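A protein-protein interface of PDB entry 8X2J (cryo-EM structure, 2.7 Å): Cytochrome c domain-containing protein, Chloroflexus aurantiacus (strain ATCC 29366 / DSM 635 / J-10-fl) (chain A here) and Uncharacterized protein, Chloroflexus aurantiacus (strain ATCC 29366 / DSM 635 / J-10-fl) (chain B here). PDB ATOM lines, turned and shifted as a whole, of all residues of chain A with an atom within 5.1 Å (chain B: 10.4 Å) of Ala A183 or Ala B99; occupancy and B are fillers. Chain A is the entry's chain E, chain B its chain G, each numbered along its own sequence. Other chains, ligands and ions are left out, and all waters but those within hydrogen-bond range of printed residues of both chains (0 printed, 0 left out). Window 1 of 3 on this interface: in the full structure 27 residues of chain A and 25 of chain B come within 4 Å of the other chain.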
ATOM      1  N   LEU A  92       6.848  11.554  -6.792  1.00  0.00           N
ATOM      2  CA  LEU A  92       5.592  11.568  -7.534  1.00  0.00           C
ATOM      3  C   LEU A  92       5.309  12.935  -8.143  1.00  0.00           C
ATOM      4  O   LEU A  92       4.750  13.015  -9.240  1.00  0.00           O
ATOM      5  CB  LEU A  92       4.443  11.145  -6.622  1.00  0.00           C
ATOM      6  CG  LEU A  92       4.046   9.671  -6.680  1.00  0.00           C
ATOM      7  CD1 LEU A  92       3.024   9.364  -5.610  1.00  0.00           C
ATOM      8  CD2 LEU A  92       3.498   9.329  -8.047  1.00  0.00           C
ATOM      9  N   ALA A 179       5.633   5.805 -11.819  1.00  0.00           N
ATOM     10  CA  ALA A 179       4.919   5.965 -10.553  1.00  0.00           C
ATOM     11  C   ALA A 179       3.728   6.907 -10.698  1.00  0.00           C
ATOM     12  O   ALA A 179       2.659   6.664 -10.122  1.00  0.00           O
ATOM     13  CB  ALA A 179       5.870   6.472  -9.473  1.00  0.00           C
ATOM     14  N   TYR A 180       3.886   7.982 -11.474  1.00  0.00           N
ATOM     15  CA  TYR A 180       2.750   8.865 -11.729  1.00  0.00           C
ATOM     16  C   TYR A 180       1.706   8.208 -12.627  1.00  0.00           C
ATOM     17  O   TYR A 180       0.521   8.546 -12.540  1.00  0.00           O
ATOM     18  CB  TYR A 180       3.216  10.184 -12.341  1.00  0.00           C
ATOM     19  CG  TYR A 180       2.102  11.198 -12.437  1.00  0.00           C
ATOM     20  CD1 TYR A 180       1.440  11.642 -11.298  1.00  0.00           C
ATOM     21  CD2 TYR A 180       1.681  11.678 -13.669  1.00  0.00           C
ATOM     22  CE1 TYR A 180       0.406  12.555 -11.384  1.00  0.00           C
ATOM     23  CE2 TYR A 180       0.654  12.595 -13.765  1.00  0.00           C
ATOM     24  CZ  TYR A 180       0.019  13.027 -12.622  1.00  0.00           C
ATOM     25  OH  TYR A 180      -1.005  13.938 -12.721  1.00  0.00           O
ATOM     26  N   ILE A 181       2.121   7.278 -13.491  1.00  0.00           N
ATOM     27  CA  ILE A 181       1.170   6.493 -14.278  1.00  0.00           C
ATOM     28  C   ILE A 181       0.328   5.616 -13.359  1.00  0.00           C
ATOM     29  O   ILE A 181      -0.897   5.515 -13.519  1.00  0.00           O
ATOM     30  CB  ILE A 181       1.917   5.664 -15.344  1.00  0.00           C
ATOM     31  CG1 ILE A 181       2.405   6.563 -16.476  1.00  0.00           C
ATOM     32  CG2 ILE A 181       1.043   4.557 -15.920  1.00  0.00           C
ATOM     33  CD1 ILE A 181       1.309   7.321 -17.150  1.00  0.00           C
ATOM     34  N   ARG A 182       0.972   4.998 -12.366  1.00  0.00           N
ATOM     35  CA  ARG A 182       0.243   4.238 -11.351  1.00  0.00           C
ATOM     36  C   ARG A 182      -0.683   5.136 -10.533  1.00  0.00           C
ATOM     37  O   ARG A 182      -1.800   4.735 -10.179  1.00  0.00           O
ATOM     38  CB  ARG A 182       1.229   3.513 -10.438  1.00  0.00           C
ATOM     39  CG  ARG A 182       1.562   2.113 -10.898  1.00  0.00           C
ATOM     40  CD  ARG A 182       0.409   1.165 -10.639  1.00  0.00           C
ATOM     41  NE  ARG A 182       0.698  -0.180 -11.118  1.00  0.00           N
ATOM     42  CZ  ARG A 182       0.412  -0.619 -12.335  1.00  0.00           C
ATOM     43  NH1 ARG A 182      -0.183   0.155 -13.226  1.00  0.00           N
ATOM     44  NH2 ARG A 182       0.727  -1.869 -12.664  1.00  0.00           N
ATOM     45  N   ALA A 183      -0.235   6.360 -10.238  1.00  0.00           N
ATOM     46  CA  ALA A 183      -1.074   7.327  -9.528  1.00  0.00           C
ATOM     47  C   ALA A 183      -2.294   7.732 -10.351  1.00  0.00           C
ATOM     48  O   ALA A 183      -3.395   7.860  -9.808  1.00  0.00           O
ATOM     49  CB  ALA A 183      -0.251   8.558  -9.154  1.00  0.00           C
ATOM     50  N   LEU A 184      -2.121   7.930 -11.660  1.00  0.00           N
ATOM     51  CA  LEU A 184      -3.248   8.268 -12.530  1.00  0.00           C
ATOM     52  C   LEU A 184      -4.205   7.092 -12.683  1.00  0.00           C
ATOM     53  O   LEU A 184      -5.424   7.284 -12.797  1.00  0.00           O
ATOM     54  CB  LEU A 184      -2.740   8.713 -13.901  1.00  0.00           C
ATOM     55  CG  LEU A 184      -2.262  10.153 -14.080  1.00  0.00           C
ATOM     56  CD1 LEU A 184      -1.622  10.314 -15.445  1.00  0.00           C
ATOM     57  CD2 LEU A 184      -3.414  11.130 -13.911  1.00  0.00           C
ATOM     58  N   GLN A 185      -3.668   5.869 -12.707  1.00  0.00           N
ATOM     59  CA  GLN A 185      -4.515   4.683 -12.759  1.00  0.00           C
ATOM     60  C   GLN A 185      -5.316   4.512 -11.476  1.00  0.00           C
ATOM     61  O   GLN A 185      -6.463   4.056 -11.524  1.00  0.00           O
ATOM     62  CB  GLN A 185      -3.667   3.443 -13.030  1.00  0.00           C
ATOM     63  CG  GLN A 185      -3.213   3.319 -14.471  1.00  0.00           C
ATOM     64  CD  GLN A 185      -2.468   2.033 -14.735  1.00  0.00           C
ATOM     65  OE1 GLN A 185      -2.288   1.212 -13.838  1.00  0.00           O
ATOM     66  NE2 GLN A 185      -2.024   1.851 -15.972  1.00  0.00           N
ATOM     67  N   LEU A 186      -4.735   4.865 -10.328  1.00  0.00           N
ATOM     68  CA  LEU A 186      -5.520   4.913  -9.097  1.00  0.00           C
ATOM     69  C   LEU A 186      -6.515   6.070  -9.112  1.00  0.00           C
ATOM     70  O   LEU A 186      -7.591   5.966  -8.510  1.00  0.00           O
ATOM     71  CB  LEU A 186      -4.600   5.024  -7.881  1.00  0.00           C
ATOM     72  CG  LEU A 186      -5.252   4.720  -6.528  1.00  0.00           C
ATOM     73  CD1 LEU A 186      -5.771   3.291  -6.488  1.00  0.00           C
ATOM     74  CD2 LEU A 186      -4.292   4.981  -5.380  1.00  0.00           C
ATOM     75  N   SER A 187      -6.163   7.173  -9.779  1.00  0.00           N
ATOM     76  CA  SER A 187      -7.044   8.336  -9.864  1.00  0.00           C
ATOM     77  C   SER A 187      -8.314   8.021 -10.639  1.00  0.00           C
ATOM     78  O   SER A 187      -9.411   8.430 -10.238  1.00  0.00           O
ATOM     79  CB  SER A 187      -6.309   9.503 -10.525  1.00  0.00           C
ATOM     80  OG  SER A 187      -5.146   9.863  -9.808  1.00  0.00           O
ATOM     81  N   LEU B  80     -11.385  17.044 -14.899  1.00  0.00           N
ATOM     82  CA  LEU B  80     -11.629  15.645 -14.570  1.00  0.00           C
ATOM     83  C   LEU B  80     -10.674  15.127 -13.502  1.00  0.00           C
ATOM     84  O   LEU B  80     -10.989  14.137 -12.834  1.00  0.00           O
ATOM     85  CB  LEU B  80     -11.520  14.785 -15.830  1.00  0.00           C
ATOM     86  CG  LEU B  80     -12.283  13.459 -15.833  1.00  0.00           C
ATOM     87  CD1 LEU B  80     -13.780  13.705 -15.947  1.00  0.00           C
ATOM     88  CD2 LEU B  80     -11.797  12.560 -16.962  1.00  0.00           C
ATOM     89  N   LEU B  81      -9.524  15.771 -13.325  1.00  0.00           N
ATOM     90  CA  LEU B  81      -8.554  15.373 -12.316  1.00  0.00           C
ATOM     91  C   LEU B  81      -8.778  16.062 -10.976  1.00  0.00           C
ATOM     92  O   LEU B  81      -7.938  15.930 -10.080  1.00  0.00           O
ATOM     93  CB  LEU B  81      -7.133  15.651 -12.812  1.00  0.00           C
ATOM     94  CG  LEU B  81      -6.497  14.586 -13.707  1.00  0.00           C
ATOM     95  CD1 LEU B  81      -5.058  14.952 -14.032  1.00  0.00           C
ATOM     96  CD2 LEU B  81      -6.576  13.213 -13.060  1.00  0.00           C
ATOM     97  N   ASN B  82      -9.877  16.798 -10.823  1.00  0.00           N
ATOM     98  CA  ASN B  82     -10.194  17.481  -9.577  1.00  0.00           C
ATOM     99  C   ASN B  82     -11.685  17.354  -9.297  1.00  0.00           C
ATOM    100  O   ASN B  82     -12.465  16.917 -10.149  1.00  0.00           O
ATOM    101  CB  ASN B  82      -9.784  18.958  -9.624  1.00  0.00           C
ATOM    102  CG  ASN B  82      -8.283  19.152  -9.534  1.00  0.00           C
ATOM    103  OD1 ASN B  82      -7.609  18.506  -8.733  1.00  0.00           O
ATOM    104  ND2 ASN B  82      -7.753  20.047 -10.357  1.00  0.00           N
ATOM    105  N   TYR B  84     -13.496  15.398  -7.596  1.00  0.00           N
ATOM    106  CA  TYR B  84     -14.008  14.009  -7.548  1.00  0.00           C
ATOM    107  C   TYR B  84     -14.861  13.763  -8.799  1.00  0.00           C
ATOM    108  O   TYR B  84     -14.503  14.233  -9.890  1.00  0.00           O
ATOM    109  CB  TYR B  84     -14.710  13.762  -6.224  1.00  0.00           C
ATOM    110  CG  TYR B  84     -13.758  13.592  -5.065  1.00  0.00           C
ATOM    111  CD1 TYR B  84     -13.280  14.694  -4.365  1.00  0.00           C
ATOM    112  CD2 TYR B  84     -13.326  12.330  -4.676  1.00  0.00           C
ATOM    113  CE1 TYR B  84     -12.402  14.545  -3.306  1.00  0.00           C
ATOM    114  CE2 TYR B  84     -12.449  12.169  -3.618  1.00  0.00           C
ATOM    115  CZ  TYR B  84     -11.992  13.280  -2.938  1.00  0.00           C
ATOM    116  OH  TYR B  84     -11.121  13.125  -1.885  1.00  0.00           O
ATOM    117  N   VAL B  92     -15.497   6.031  -8.948  1.00  0.00           N
ATOM    118  CA  VAL B  92     -15.354   7.402  -8.468  1.00  0.00           C
ATOM    119  C   VAL B  92     -13.954   7.886  -8.826  1.00  0.00           C
ATOM    120  O   VAL B  92     -13.017   7.090  -8.941  1.00  0.00           O
ATOM    121  CB  VAL B  92     -15.646   7.475  -6.943  1.00  0.00           C
ATOM    122  CG1 VAL B  92     -14.611   6.699  -6.126  1.00  0.00           C
ATOM    123  CG2 VAL B  92     -15.823   8.913  -6.441  1.00  0.00           C
ATOM    124  N   HIS B  93     -13.821   9.194  -9.044  1.00  0.00           N
ATOM    125  CA  HIS B  93     -12.510   9.806  -9.206  1.00  0.00           C
ATOM    126  C   HIS B  93     -11.808   9.926  -7.861  1.00  0.00           C
ATOM    127  O   HIS B  93     -12.444  10.020  -6.807  1.00  0.00           O
ATOM    128  CB  HIS B  93     -12.613  11.206  -9.814  1.00  0.00           C
ATOM    129  CG  HIS B  93     -13.313  11.259 -11.133  1.00  0.00           C
ATOM    130  ND1 HIS B  93     -13.932  12.400 -11.594  1.00  0.00           N
ATOM    131  CD2 HIS B  93     -13.485  10.323 -12.094  1.00  0.00           C
ATOM    132  CE1 HIS B  93     -14.462  12.162 -12.780  1.00  0.00           C
ATOM    133  NE2 HIS B  93     -14.203  10.909 -13.108  1.00  0.00           N
ATOM    134  N   ILE B  94     -10.482   9.919  -7.907  1.00  0.00           N
ATOM    135  CA  ILE B  94      -9.642  10.370  -6.807  1.00  0.00           C
ATOM    136  C   ILE B  94      -8.763  11.479  -7.372  1.00  0.00           C
ATOM    137  O   ILE B  94      -8.028  11.250  -8.336  1.00  0.00           O
ATOM    138  CB  ILE B  94      -8.785   9.243  -6.205  1.00  0.00           C
ATOM    139  CG1 ILE B  94      -9.623   7.987  -5.958  1.00  0.00           C
ATOM    140  CG2 ILE B  94      -8.172   9.696  -4.896  1.00  0.00           C
ATOM    141  CD1 ILE B  94      -8.821   6.800  -5.475  1.00  0.00           C
ATOM    142  N   PRO B  95      -8.815  12.693  -6.836  1.00  0.00           N
ATOM    143  CA  PRO B  95      -8.137  13.824  -7.476  1.00  0.00           C
ATOM    144  C   PRO B  95      -6.626  13.789  -7.277  1.00  0.00           C
ATOM    145  O   PRO B  95      -6.082  13.009  -6.496  1.00  0.00           O
ATOM    146  CB  PRO B  95      -8.750  15.051  -6.781  1.00  0.00           C
ATOM    147  CG  PRO B  95      -9.938  14.535  -6.021  1.00  0.00           C
ATOM    148  CD  PRO B  95      -9.609  13.123  -5.676  1.00  0.00           C
ATOM    149  N   ILE B  96      -5.952  14.657  -8.037  1.00  0.00           N
ATOM    150  CA  ILE B  96      -4.531  14.916  -7.839  1.00  0.00           C
ATOM    151  C   ILE B  96      -4.333  15.574  -6.476  1.00  0.00           C
ATOM    152  O   ILE B  96      -5.209  16.300  -5.983  1.00  0.00           O
ATOM    153  CB  ILE B  96      -4.001  15.785  -8.997  1.00  0.00           C
ATOM    154  CG1 ILE B  96      -4.393  15.162 -10.335  1.00  0.00           C
ATOM    155  CG2 ILE B  96      -2.482  15.932  -8.976  1.00  0.00           C
ATOM    156  CD1 ILE B  96      -3.811  13.777 -10.555  1.00  0.00           C
ATOM    157  N   ASP B  97      -3.189  15.263  -5.843  1.00  0.00           N
ATOM    158  CA  ASP B  97      -2.781  15.556  -4.463  1.00  0.00           C
ATOM    159  C   ASP B  97      -3.620  14.776  -3.452  1.00  0.00           C
ATOM    160  O   ASP B  97      -3.557  15.046  -2.246  1.00  0.00           O
ATOM    161  CB  ASP B  97      -2.788  17.064  -4.148  1.00  0.00           C
ATOM    162  CG  ASP B  97      -1.854  17.441  -3.007  1.00  0.00           C
ATOM    163  OD1 ASP B  97      -0.624  17.461  -3.227  1.00  0.00           O
ATOM    164  OD2 ASP B  97      -2.350  17.720  -1.895  1.00  0.00           O
ATOM    165  N   ARG B  98      -4.406  13.805  -3.913  1.00  0.00           N
ATOM    166  CA  ARG B  98      -5.044  12.818  -3.054  1.00  0.00           C
ATOM    167  C   ARG B  98      -4.633  11.403  -3.422  1.00  0.00           C
ATOM    168  O   ARG B  98      -4.193  10.643  -2.550  1.00  0.00           O
ATOM    169  CB  ARG B  98      -6.573  12.962  -3.126  1.00  0.00           C
ATOM    170  CG  ARG B  98      -7.332  12.080  -2.150  1.00  0.00           C
ATOM    171  CD  ARG B  98      -7.563  12.781  -0.824  1.00  0.00           C
ATOM    172  NE  ARG B  98      -8.223  11.908   0.140  1.00  0.00           N
ATOM    173  CZ  ARG B  98      -7.602  11.273   1.123  1.00  0.00           C
ATOM    174  NH1 ARG B  98      -6.296  11.388   1.305  1.00  0.00           N
ATOM    175  NH2 ARG B  98      -8.308  10.500   1.944  1.00  0.00           N
ATOM    176  N   ALA B  99      -4.728  11.041  -4.706  1.00  0.00           N
ATOM    177  CA  ALA B  99      -4.350   9.699  -5.139  1.00  0.00           C
ATOM    178  C   ALA B  99      -2.848   9.480  -5.057  1.00  0.00           C
ATOM    179  O   ALA B  99      -2.403   8.353  -4.821  1.00  0.00           O
ATOM    180  CB  ALA B  99      -4.841   9.443  -6.561  1.00  0.00           C
ATOM    181  N   MET B 100      -2.055  10.540  -5.239  1.00  0.00           N
ATOM    182  CA  MET B 100      -0.617  10.439  -5.009  1.00  0.00           C
ATOM    183  C   MET B 100      -0.317  10.171  -3.539  1.00  0.00           C
ATOM    184  O   MET B 100       0.599   9.405  -3.213  1.00  0.00           O
ATOM    185  CB  MET B 100       0.075  11.717  -5.482  1.00  0.00           C
ATOM    186  CG  MET B 100      -0.245  12.087  -6.923  1.00  0.00           C
ATOM    187  SD  MET B 100       0.100  13.811  -7.320  1.00  0.00           S
ATOM    188  CE  MET B 100       1.883  13.831  -7.218  1.00  0.00           C
ATOM    189  N   ASP B 101      -1.100  10.772  -2.639  1.00  0.00           N
ATOM    190  CA  ASP B 101      -0.940  10.506  -1.212  1.00  0.00           C
ATOM    191  C   ASP B 101      -1.352   9.083  -0.857  1.00  0.00           C
ATOM    192  O   ASP B 101      -0.711   8.442  -0.018  1.00  0.00           O
ATOM    193  CB  ASP B 101      -1.741  11.521  -0.399  1.00  0.00           C
ATOM    194  CG  ASP B 101      -1.103  12.893  -0.393  1.00  0.00           C
ATOM    195  OD1 ASP B 101       0.124  12.978  -0.609  1.00  0.00           O
ATOM    196  OD2 ASP B 101      -1.826  13.888  -0.172  1.00  0.00           O
ATOM    197  N   LEU B 102      -2.412   8.567  -1.490  1.00  0.00           N
ATOM    198  CA  LEU B 102      -2.783   7.165  -1.287  1.00  0.00           C
ATOM    199  C   LEU B 102      -1.730   6.210  -1.844  1.00  0.00           C
ATOM    200  O   LEU B 102      -1.480   5.154  -1.254  1.00  0.00           O
ATOM    201  CB  LEU B 102      -4.154   6.863  -1.899  1.00  0.00           C
ATOM    202  CG  LEU B 102      -5.445   7.079  -1.093  1.00  0.00           C
ATOM    203  CD1 LEU B 102      -5.457   6.124   0.093  1.00  0.00           C
ATOM    204  CD2 LEU B 102      -5.670   8.499  -0.609  1.00  0.00           C
ATOM    205  N   ILE B 103      -1.106   6.564  -2.974  1.00  0.00           N
ATOM    206  CA  ILE B 103      -0.028   5.752  -3.538  1.00  0.00           C
ATOM    207  C   ILE B 103       1.176   5.735  -2.599  1.00  0.00           C
ATOM    208  O   ILE B 103       1.779   4.680  -2.359  1.00  0.00           O
ATOM    209  CB  ILE B 103       0.339   6.270  -4.947  1.00  0.00           C
ATOM    210  CG1 ILE B 103      -0.676   5.777  -5.981  1.00  0.00           C
ATOM    211  CG2 ILE B 103       1.742   5.845  -5.369  1.00  0.00           C
ATOM    212  CD1 ILE B 103      -0.639   4.282  -6.223  1.00  0.00           C
ATOM    213  N   VAL B 104       1.513   6.895  -2.026  1.00  0.00           N
ATOM    214  CA  VAL B 104       2.616   6.991  -1.066  1.00  0.00           C
ATOM    215  C   VAL B 104       2.307   6.193   0.199  1.00  0.00           C
ATOM    216  O   VAL B 104       3.169   5.472   0.723  1.00  0.00           O
ATOM    217  CB  VAL B 104       2.912   8.476  -0.763  1.00  0.00           C
ATOM    218  CG1 VAL B 104       3.685   8.654   0.539  1.00  0.00           C
ATOM    219  CG2 VAL B 104       3.676   9.104  -1.913  1.00  0.00           C
ATOM    220  N   GLU B 105       1.062   6.274   0.686  1.00  0.00           N
ATOM    221  CA  GLU B 105       0.681   5.572   1.910  1.00  0.00           C
ATOM    222  C   GLU B 105       0.652   4.059   1.717  1.00  0.00           C
ATOM    223  O   GLU B 105       1.134   3.312   2.575  1.00  0.00           O
ATOM    224  CB  GLU B 105      -0.679   6.070   2.396  1.00  0.00           C
ATOM    225  CG  GLU B 105      -0.627   7.378   3.165  1.00  0.00           C
ATOM    226  CD  GLU B 105      -1.988   8.037   3.276  1.00  0.00           C
ATOM    227  OE1 GLU B 105      -3.003   7.346   3.050  1.00  0.00           O
ATOM    228  OE2 GLU B 105      -2.042   9.243   3.590  1.00  0.00           O
ATOM    229  N   ARG B 106       0.092   3.583   0.603  1.00  0.00           N
ATOM    230  CA  ARG B 106       0.010   2.149   0.366  1.00  0.00           C
ATOM    231  C   ARG B 106       1.305   1.562  -0.177  1.00  0.00           C
ATOM    232  O   ARG B 106       1.459   0.335  -0.168  1.00  0.00           O
ATOM    233  CB  ARG B 106      -1.148   1.838  -0.588  1.00  0.00           C
ATOM    234  CG  ARG B 106      -0.821   2.003  -2.062  1.00  0.00           C
ATOM    235  CD  ARG B 106      -2.060   1.793  -2.916  1.00  0.00           C
ATOM    236  NE  ARG B 106      -3.228   2.455  -2.345  1.00  0.00           N
ATOM    237  CZ  ARG B 106      -4.477   2.241  -2.736  1.00  0.00           C
ATOM    238  NH1 ARG B 106      -4.761   1.382  -3.700  1.00  0.00           N
ATOM    239  NH2 ARG B 106      -5.464   2.906  -2.143  1.00  0.00           N
ATOM    240  N   GLY B 107       2.235   2.394  -0.643  1.00  0.00           N
ATOM    241  CA  GLY B 107       3.510   1.911  -1.124  1.00  0.00           C
ATOM    242  C   GLY B 107       3.423   1.308  -2.514  1.00  0.00           C
ATOM    243  O   GLY B 107       2.365   1.209  -3.136  1.00  0.00           O
ATOM    244  N   LEU B 108       4.587   0.902  -3.006  1.00  0.00           N
ATOM    245  CA  LEU B 108       4.734   0.213  -4.275  1.00  0.00           C
ATOM    246  C   LEU B 108       5.654  -0.983  -4.083  1.00  0.00           C
ATOM    247  O   LEU B 108       6.483  -0.981  -3.166  1.00  0.00           O
ATOM    248  CB  LEU B 108       5.303   1.153  -5.350  1.00  0.00           C
ATOM    249  CG  LEU B 108       4.303   2.145  -5.952  1.00  0.00           C
ATOM    250  CD1 LEU B 108       4.964   3.008  -7.013  1.00  0.00           C
ATOM    251  CD2 LEU B 108       3.095   1.418  -6.525  1.00  0.00           C
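Of the 21 printed residues of chain B, 10 touch a printed residue of chain A. Printed residues of chain B that touch a printed residue of chain A: Leu B81, His B93, Ile B94, Ile B96, Ala B99, Met B100, Leu B102, Ile B103, Val B104 and Arg B106. Hydrophobic or aromatic side chains of chain B within 4 Å of the printed part of chain A: Leu B81, Ile B94, Ile B96, Ala B99, Met B100, Leu B102, Ile B103 and Val B104. Of the 10 printed residues of chain A, 6 touch a printed residue of chain B. Printed residues of chain A that touch a printed residue of chain B: Leu A92, Tyr A180, Ala A183, Leu A184, Leu A186 and Ser A187. Hydrophobic or aromatic side chains of chain A within 4 Å of the printed part of chain B: Leu A92, Tyr A180, Leu A184 and Leu A186. Along chain A the printed residues that touch a printed residue of chain B span positions 92 to 187. Among the printed residues, 15 pairs touch across the chains.
Of the printed residues of chain B, Leu A92 touches Met B100 (3.4 Å), Ile B103 (3.8 Å) and Val B104 (3.8 Å). Of chain B, only Ala B99 and Ile B103 come within 4 Å of Ala A183. Of chain B, only Leu B81 comes within 4 Å of Leu A184. Leu A186 touches just these residues of chain B: Ile B94, Ala B99, Leu B102, Ile B103 and Arg B106. Of chain B, only His B93 (3.5 Å), Ile B94 (3.0 Å) and Ala B99 (3.3 Å) come within 4 Å of Ser A187. Ala B99 touches just these residues of chain A: Ala A183 (3.9 Å), Leu A186 (3.9 Å) and Ser A187 (3.3 Å). Printed residues of chain A within 4 Å of Leu B102: Leu A186. The nearest residue of chain B that does not touch Ala A183 is Met B100 (4.2 Å). The nearest printed residue of chain A that does not touch Ala B99 is Leu A92 (5.6 Å). The nearest printed residue of chain B that does not touch Tyr A180 is Met B100 (4.3 Å).
A ring nitrogen (ND1) of His B93 lies within hydrogen-bond range of the backbone carbonyl oxygen of Tyr B84 (2.6 Å). NE of Arg B106 sits close to O of Leu B102 (3.4 Å). O of Ala A183 lies within hydrogen-bond range of OG of Ser A187 (2.7 Å). The backbone NH (N) of Ile B96 sits at hydrogen-bond distance from the backbone carbonyl oxygen (O) of Leu B81 (3.1 Å).
N of Ile B94 sits at hydrogen-bond distance from O of Ser A187 (3.0 Å).
O of Met B100 touches CD1 of Leu A92, 3.4 Å away. CG2 of Ile B103 touches CD1 of Leu A92, 3.8 Å away. Ile B96 touches Tyr A180 (CD1 to OH, 3.5 Å). CA of Ala A183 touches CG1 of Ile B103, 3.9 Å away. Leu A184 touches Leu B81 (CD2 to CD2, 3.9 Å). Leu A186 touches Ile B94 (O to CD1, 3.4 Å). CD2 of Leu A186 touches O of Ala B99 (3.9 Å). Leu A186 touches Leu B102 (CD2 to CB, 3.96 Å). Ile B103 touches Leu A186. His B93 touches Ser A187 (CA to O, 3.5 Å).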
